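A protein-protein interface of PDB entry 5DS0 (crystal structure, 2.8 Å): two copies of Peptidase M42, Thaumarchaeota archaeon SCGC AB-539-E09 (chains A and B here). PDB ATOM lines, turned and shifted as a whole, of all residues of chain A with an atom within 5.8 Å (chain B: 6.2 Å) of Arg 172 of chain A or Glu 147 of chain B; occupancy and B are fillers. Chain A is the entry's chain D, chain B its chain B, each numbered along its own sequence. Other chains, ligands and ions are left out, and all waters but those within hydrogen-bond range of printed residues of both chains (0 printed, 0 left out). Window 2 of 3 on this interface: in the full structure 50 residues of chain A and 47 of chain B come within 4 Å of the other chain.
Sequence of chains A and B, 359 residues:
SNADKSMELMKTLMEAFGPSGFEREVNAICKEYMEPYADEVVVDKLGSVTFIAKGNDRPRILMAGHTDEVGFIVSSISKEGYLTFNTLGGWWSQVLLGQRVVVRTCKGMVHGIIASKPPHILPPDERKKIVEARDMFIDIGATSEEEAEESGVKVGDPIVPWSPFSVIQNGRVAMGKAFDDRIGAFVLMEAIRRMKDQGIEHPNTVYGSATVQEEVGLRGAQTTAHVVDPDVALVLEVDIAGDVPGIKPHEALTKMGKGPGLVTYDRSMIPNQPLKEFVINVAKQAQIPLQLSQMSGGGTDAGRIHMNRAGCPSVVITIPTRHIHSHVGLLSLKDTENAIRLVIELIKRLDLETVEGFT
CD1 of Ile 168 of chain A touches O of Ile 140 of chain B (3.8 Å).
Gln 169 of chain A touches Gly 141 of chain B (CG to O, 3.5 Å).
Ala 142 of chain B touches Gln 169 of chain A (N to NE2, 3.8 Å).
Val 173 of chain A touches Gly 141 of chain B (CG2 to O, 3.9 Å).
The backbone carbonyl oxygen (O) of Ile 140 of chain B sits at hydrogen-bond distance from the side-chain amide nitrogen (NE2) of Gln 169 of chain A, at 2.8 Å.
The side-chain carboxylate (OE1) of Glu 147 of chain B is in salt-bridge range of the guanidinium group (NH2) of Arg 172 of chain A (3.9 Å).
No position is printed for both chains.
Of the 6 pairs that touch across the chains among the printed residues, none has its exchanged pair printed and touching as well.
The side-chain amide oxygen (OE1) of Gln 169 of chain A sits at hydrogen-bond distance from the guanidinium group (NH2) of Arg 172 of chain A (2.8 Å).
O of Arg 172 of chain A is in hydrogen-bond range of N of Leu 333 of chain A, 3.1 Å away.
The backbone NH (N) of Glu 147 of chain B lies within hydrogen-bond range of the side-chain hydroxyl (OG) of Ser 144 of chain B, 3.2 Å away.
OE2 of Glu 147 of chain B is in hydrogen-bond range of OG1 of Thr 143 of chain B, at 2.9 Å.
N of Ile 168 of chain A is in hydrogen-bond range of O of Val 173 of chain A.
Of the printed residues of chain B, Ile 168 of chain A touches Ile 140 (3.8 Å).
Of chain B, only Glu 147 (3.7 Å) comes within 4 Å of Arg 172 of chain A.
Printed residues of chain B within 4 Å of Val 173 of chain A: Gly 141 (3.9 Å).
Of the printed residues of chain A, Ile 140 of chain B touches Ile 168 and Gln 169.
Printed residues of chain A within 4 Å of Gly 141 of chain B: Gln 169 and Val 173.
Of the printed residues of chain A, Ala 142 of chain B touches Gln 169 (3.8 Å).
The nearest residue of chain B that does not touch Arg 172 of chain A is Glu 150 of chain B (5.3 Å).
The nearest residue of chain A that does not touch Glu 147 of chain B is Gln 169 of chain A (4.1 Å).
Of the 13 printed residues of chain B, 4 touch a printed residue of chain A.
Along chain A the printed residues that touch a printed residue of chain B span positions 168 to 173.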
ATOM      1  N   VAL A 167       1.272  -7.068  22.074  1.00  0.00           N
ATOM      2  CA  VAL A 167       0.790  -5.844  22.693  1.00  0.00           C
ATOM      3  C   VAL A 167       0.269  -4.913  21.610  1.00  0.00           C
ATOM      4  O   VAL A 167       0.892  -4.777  20.555  1.00  0.00           O
ATOM      5  CB  VAL A 167       1.902  -5.136  23.462  1.00  0.00           C
ATOM      6  CG1 VAL A 167       1.356  -3.878  24.120  1.00  0.00           C
ATOM      7  CG2 VAL A 167       2.492  -6.057  24.519  1.00  0.00           C
ATOM      8  N   ILE A 168      -0.870  -4.284  21.866  1.00  0.00           N
ATOM      9  CA  ILE A 168      -1.491  -3.384  20.909  1.00  0.00           C
ATOM     10  C   ILE A 168      -1.780  -2.039  21.554  1.00  0.00           C
ATOM     11  O   ILE A 168      -1.375  -1.791  22.698  1.00  0.00           O
ATOM     12  CB  ILE A 168      -2.777  -3.982  20.319  1.00  0.00           C
ATOM     13  CG1 ILE A 168      -3.775  -4.340  21.423  1.00  0.00           C
ATOM     14  CG2 ILE A 168      -2.438  -5.206  19.483  1.00  0.00           C
ATOM     15  CD1 ILE A 168      -5.159  -4.672  20.904  1.00  0.00           C
ATOM     16  N   GLN A 169      -2.428  -1.149  20.801  1.00  0.00           N
ATOM     17  CA  GLN A 169      -2.745   0.198  21.285  1.00  0.00           C
ATOM     18  C   GLN A 169      -1.500   0.933  21.801  1.00  0.00           C
ATOM     19  O   GLN A 169      -1.458   1.361  22.962  1.00  0.00           O
ATOM     20  CB  GLN A 169      -3.811   0.114  22.380  1.00  0.00           C
ATOM     21  CG  GLN A 169      -5.183  -0.246  21.856  1.00  0.00           C
ATOM     22  CD  GLN A 169      -5.837   0.878  21.097  1.00  0.00           C
ATOM     23  OE1 GLN A 169      -5.460   2.031  21.232  1.00  0.00           O
ATOM     24  NE2 GLN A 169      -6.809   0.543  20.280  1.00  0.00           N
ATOM     25  N   ASN A 170      -0.480   1.025  20.948  1.00  0.00           N
ATOM     26  CA  ASN A 170       0.736   1.750  21.282  1.00  0.00           C
ATOM     27  C   ASN A 170       1.313   1.311  22.610  1.00  0.00           C
ATOM     28  O   ASN A 170       1.579   2.140  23.479  1.00  0.00           O
ATOM     29  CB  ASN A 170       0.439   3.241  21.333  1.00  0.00           C
ATOM     30  CG  ASN A 170      -0.303   3.713  20.106  1.00  0.00           C
ATOM     31  OD1 ASN A 170      -1.532   3.866  20.115  1.00  0.00           O
ATOM     32  ND2 ASN A 170       0.437   3.951  19.032  1.00  0.00           N
ATOM     33  N   GLY A 171       1.444   0.005  22.792  1.00  0.00           N
ATOM     34  CA  GLY A 171       2.079  -0.528  23.986  1.00  0.00           C
ATOM     35  C   GLY A 171       1.242  -0.570  25.253  1.00  0.00           C
ATOM     36  O   GLY A 171       1.754  -0.952  26.294  1.00  0.00           O
ATOM     37  N   ARG A 172      -0.038  -0.218  25.174  1.00  0.00           N
ATOM     38  CA  ARG A 172      -0.894  -0.069  26.367  1.00  0.00           C
ATOM     39  C   ARG A 172      -1.662  -1.331  26.770  1.00  0.00           C
ATOM     40  O   ARG A 172      -1.978  -1.508  27.949  1.00  0.00           O
ATOM     41  CB  ARG A 172      -1.925   1.049  26.148  1.00  0.00           C
ATOM     42  CG  ARG A 172      -1.421   2.452  26.400  1.00  0.00           C
ATOM     43  CD  ARG A 172      -2.556   3.475  26.419  1.00  0.00           C
ATOM     44  NE  ARG A 172      -3.493   3.341  25.295  1.00  0.00           N
ATOM     45  CZ  ARG A 172      -3.369   3.908  24.088  1.00  0.00           C
ATOM     46  NH1 ARG A 172      -2.327   4.687  23.798  1.00  0.00           N
ATOM     47  NH2 ARG A 172      -4.304   3.682  23.164  1.00  0.00           N
ATOM     48  N   VAL A 173      -1.978  -2.181  25.792  1.00  0.00           N
ATOM     49  CA  VAL A 173      -2.920  -3.274  25.983  1.00  0.00           C
ATOM     50  C   VAL A 173      -2.347  -4.595  25.508  1.00  0.00           C
ATOM     51  O   VAL A 173      -1.951  -4.722  24.355  1.00  0.00           O
ATOM     52  CB  VAL A 173      -4.222  -3.018  25.185  1.00  0.00           C
ATOM     53  CG1 VAL A 173      -5.145  -4.231  25.226  1.00  0.00           C
ATOM     54  CG2 VAL A 173      -4.955  -1.784  25.705  1.00  0.00           C
ATOM     55  N   ALA A 174      -2.388  -5.597  26.379  1.00  0.00           N
ATOM     56  CA  ALA A 174      -1.869  -6.929  26.073  1.00  0.00           C
ATOM     57  C   ALA A 174      -2.952  -7.821  25.476  1.00  0.00           C
ATOM     58  O   ALA A 174      -4.097  -7.775  25.904  1.00  0.00           O
ATOM     59  CB  ALA A 174      -1.327  -7.563  27.333  1.00  0.00           C
ATOM     60  N   LEU A 331      -6.096  -7.064  28.213  1.00  0.00           N
ATOM     61  CA  LEU A 331      -6.031  -6.362  29.488  1.00  0.00           C
ATOM     62  C   LEU A 331      -5.071  -5.207  29.422  1.00  0.00           C
ATOM     63  O   LEU A 331      -4.263  -5.113  28.498  1.00  0.00           O
ATOM     64  CB  LEU A 331      -5.686  -7.305  30.636  1.00  0.00           C
ATOM     65  CG  LEU A 331      -4.397  -8.102  30.609  1.00  0.00           C
ATOM     66  CD1 LEU A 331      -3.176  -7.232  30.871  1.00  0.00           C
ATOM     67  CD2 LEU A 331      -4.449  -9.190  31.662  1.00  0.00           C
ATOM     68  N   SER A 332      -5.184  -4.313  30.398  1.00  0.00           N
ATOM     69  CA  SER A 332      -4.366  -3.091  30.452  1.00  0.00           C
ATOM     70  C   SER A 332      -3.081  -3.311  31.242  1.00  0.00           C
ATOM     71  O   SER A 332      -3.117  -3.748  32.378  1.00  0.00           O
ATOM     72  CB  SER A 332      -5.164  -1.952  31.098  1.00  0.00           C
ATOM     73  OG  SER A 332      -4.328  -0.888  31.527  1.00  0.00           O
ATOM     74  N   LEU A 333      -1.946  -2.968  30.645  1.00  0.00           N
ATOM     75  CA  LEU A 333      -0.658  -3.060  31.345  1.00  0.00           C
ATOM     76  C   LEU A 333      -0.550  -2.066  32.495  1.00  0.00           C
ATOM     77  O   LEU A 333       0.142  -2.324  33.468  1.00  0.00           O
ATOM     78  CB  LEU A 333       0.497  -2.838  30.372  1.00  0.00           C
ATOM     79  CG  LEU A 333       0.610  -3.928  29.316  1.00  0.00           C
ATOM     80  CD1 LEU A 333       1.732  -3.597  28.367  1.00  0.00           C
ATOM     81  CD2 LEU A 333       0.836  -5.299  29.956  1.00  0.00           C
ATOM     82  N   LYS A 334      -1.235  -0.936  32.362  1.00  0.00           N
ATOM     83  CA  LYS A 334      -1.318   0.046  33.417  1.00  0.00           C
ATOM     84  C   LYS A 334      -2.064  -0.497  34.638  1.00  0.00           C
ATOM     85  O   LYS A 334      -1.602  -0.331  35.761  1.00  0.00           O
ATOM     86  CB  LYS A 334      -2.013   1.286  32.895  1.00  0.00           C
ATOM     87  CG  LYS A 334      -1.967   2.451  33.851  1.00  0.00           C
ATOM     88  CD  LYS A 334      -2.922   3.554  33.429  1.00  0.00           C
ATOM     89  CE  LYS A 334      -2.936   4.660  34.480  1.00  0.00           C
ATOM     90  NZ  LYS A 334      -4.040   5.632  34.246  1.00  0.00           N
ATOM     91  N   ILE B 140     -11.106  -3.466  19.449  1.00  0.00           N
ATOM     92  CA  ILE B 140      -9.741  -3.158  19.042  1.00  0.00           C
ATOM     93  C   ILE B 140      -8.916  -2.641  20.215  1.00  0.00           C
ATOM     94  O   ILE B 140      -7.846  -2.064  20.010  1.00  0.00           O
ATOM     95  CB  ILE B 140      -9.694  -2.155  17.871  1.00  0.00           C
ATOM     96  CG1 ILE B 140     -10.400  -0.857  18.241  1.00  0.00           C
ATOM     97  CG2 ILE B 140     -10.345  -2.757  16.639  1.00  0.00           C
ATOM     98  CD1 ILE B 140     -10.080   0.288  17.313  1.00  0.00           C
ATOM     99  N   GLY B 141      -9.405  -2.877  21.432  1.00  0.00           N
ATOM    100  CA  GLY B 141      -8.697  -2.484  22.640  1.00  0.00           C
ATOM    101  C   GLY B 141      -8.872  -1.011  22.991  1.00  0.00           C
ATOM    102  O   GLY B 141      -8.128  -0.475  23.822  1.00  0.00           O
ATOM    103  N   ALA B 142      -9.859  -0.364  22.374  1.00  0.00           N
ATOM    104  CA  ALA B 142     -10.089   1.045  22.602  1.00  0.00           C
ATOM    105  C   ALA B 142     -11.039   1.208  23.785  1.00  0.00           C
ATOM    106  O   ALA B 142     -11.796   0.296  24.100  1.00  0.00           O
ATOM    107  CB  ALA B 142     -10.662   1.688  21.362  1.00  0.00           C
ATOM    108  N   THR B 143     -10.969   2.365  24.445  1.00  0.00           N
ATOM    109  CA  THR B 143     -11.791   2.657  25.623  1.00  0.00           C
ATOM    110  C   THR B 143     -12.741   3.833  25.401  1.00  0.00           C
ATOM    111  O   THR B 143     -13.443   4.227  26.320  1.00  0.00           O
ATOM    112  CB  THR B 143     -10.918   2.946  26.864  1.00  0.00           C
ATOM    113  OG1 THR B 143     -10.014   4.010  26.570  1.00  0.00           O
ATOM    114  CG2 THR B 143     -10.107   1.720  27.254  1.00  0.00           C
ATOM    115  N   SER B 144     -12.780   4.369  24.182  1.00  0.00           N
ATOM    116  CA  SER B 144     -13.658   5.492  23.848  1.00  0.00           C
ATOM    117  C   SER B 144     -13.687   5.703  22.341  1.00  0.00           C
ATOM    118  O   SER B 144     -12.774   5.289  21.633  1.00  0.00           O
ATOM    119  CB  SER B 144     -13.159   6.774  24.512  1.00  0.00           C
ATOM    120  OG  SER B 144     -11.901   7.166  23.991  1.00  0.00           O
ATOM    121  N   GLU B 145     -14.730   6.365  21.855  1.00  0.00           N
ATOM    122  CA  GLU B 145     -14.847   6.702  20.430  1.00  0.00           C
ATOM    123  C   GLU B 145     -13.619   7.415  19.889  1.00  0.00           C
ATOM    124  O   GLU B 145     -13.234   7.259  18.745  1.00  0.00           O
ATOM    125  CB  GLU B 145     -16.086   7.560  20.191  1.00  0.00           C
ATOM    126  CG  GLU B 145     -16.300   7.980  18.739  1.00  0.00           C
ATOM    127  CD  GLU B 145     -17.632   8.678  18.498  1.00  0.00           C
ATOM    128  OE1 GLU B 145     -18.482   8.721  19.428  1.00  0.00           O
ATOM    129  OE2 GLU B 145     -17.825   9.194  17.379  1.00  0.00           O
ATOM    130  N   GLU B 146     -12.988   8.213  20.718  1.00  0.00           N
ATOM    131  CA  GLU B 146     -11.814   8.936  20.272  1.00  0.00           C
ATOM    132  C   GLU B 146     -10.599   8.070  20.152  1.00  0.00           C
ATOM    133  O   GLU B 146      -9.829   8.251  19.242  1.00  0.00           O
ATOM    134  CB  GLU B 146     -11.485   9.819  21.356  1.00  0.00           C
ATOM    135  CG  GLU B 146     -10.253  10.620  21.243  1.00  0.00           C
ATOM    136  CD  GLU B 146     -10.377  12.088  21.658  1.00  0.00           C
ATOM    137  OE1 GLU B 146     -11.438  12.741  21.531  1.00  0.00           O
ATOM    138  OE2 GLU B 146      -9.357  12.632  22.070  1.00  0.00           O
ATOM    139  N   GLU B 147     -10.378   7.233  21.164  1.00  0.00           N
ATOM    140  CA  GLU B 147      -9.213   6.372  21.192  1.00  0.00           C
ATOM    141  C   GLU B 147      -9.269   5.449  19.969  1.00  0.00           C
ATOM    142  O   GLU B 147      -8.240   5.053  19.413  1.00  0.00           O
ATOM    143  CB  GLU B 147      -9.176   5.607  22.519  1.00  0.00           C
ATOM    144  CG  GLU B 147      -7.876   4.884  22.807  1.00  0.00           C
ATOM    145  CD  GLU B 147      -7.738   4.482  24.271  1.00  0.00           C
ATOM    146  OE1 GLU B 147      -7.326   5.340  25.071  1.00  0.00           O
ATOM    147  OE2 GLU B 147      -7.993   3.310  24.620  1.00  0.00           O
ATOM    148  N   ALA B 148     -10.487   5.137  19.541  1.00  0.00           N
ATOM    149  CA  ALA B 148     -10.708   4.332  18.345  1.00  0.00           C
ATOM    150  C   ALA B 148     -10.361   5.094  17.092  1.00  0.00           C
ATOM    151  O   ALA B 148      -9.741   4.551  16.192  1.00  0.00           O
ATOM    152  CB  ALA B 148     -12.159   3.884  18.275  1.00  0.00           C
ATOM    153  N   GLU B 149     -10.814   6.346  17.026  1.00  0.00           N
ATOM    154  CA  GLU B 149     -10.516   7.211  15.892  1.00  0.00           C
ATOM    155  C   GLU B 149      -9.006   7.414  15.728  1.00  0.00           C
ATOM    156  O   GLU B 149      -8.523   7.432  14.605  1.00  0.00           O
ATOM    157  CB  GLU B 149     -11.249   8.551  16.023  1.00  0.00           C
ATOM    158  CG  GLU B 149     -12.662   8.545  15.444  1.00  0.00           C
ATOM    159  CD  GLU B 149     -13.574   9.607  16.052  1.00  0.00           C
ATOM    160  OE1 GLU B 149     -13.072  10.595  16.644  1.00  0.00           O
ATOM    161  OE2 GLU B 149     -14.810   9.454  15.943  1.00  0.00           O
ATOM    162  N   GLU B 150      -8.271   7.536  16.835  1.00  0.00           N
ATOM    163  CA  GLU B 150      -6.814   7.695  16.794  1.00  0.00           C
ATOM    164  C   GLU B 150      -6.091   6.584  16.050  1.00  0.00           C
ATOM    165  O   GLU B 150      -5.045   6.805  15.457  1.00  0.00           O
ATOM    166  CB  GLU B 150      -6.240   7.801  18.198  1.00  0.00           C
ATOM    167  CG  GLU B 150      -6.338   9.197  18.795  1.00  0.00           C
ATOM    168  CD  GLU B 150      -6.070   9.208  20.304  1.00  0.00           C
ATOM    169  OE1 GLU B 150      -5.297   8.341  20.807  1.00  0.00           O
ATOM    170  OE2 GLU B 150      -6.633  10.085  20.995  1.00  0.00           O
ATOM    171  N   SER B 151      -6.656   5.393  16.057  1.00  0.00           N
ATOM    172  CA  SER B 151      -6.108   4.269  15.295  1.00  0.00           C
ATOM    173  C   SER B 151      -6.278   4.410  13.768  1.00  0.00           C
ATOM    174  O   SER B 151      -5.612   3.716  13.016  1.00  0.00           O
ATOM    175  CB  SER B 151      -6.825   3.007  15.736  1.00  0.00           C
ATOM    176  OG  SER B 151      -8.122   3.014  15.174  1.00  0.00           O
ATOM    177  N   GLY B 152      -7.193   5.272  13.331  1.00  0.00           N
ATOM    178  CA  GLY B 152      -7.369   5.586  11.917  1.00  0.00           C
ATOM    179  C   GLY B 152      -8.633   5.039  11.282  1.00  0.00           C
ATOM    180  O   GLY B 152      -8.887   5.226  10.089  1.00  0.00           O
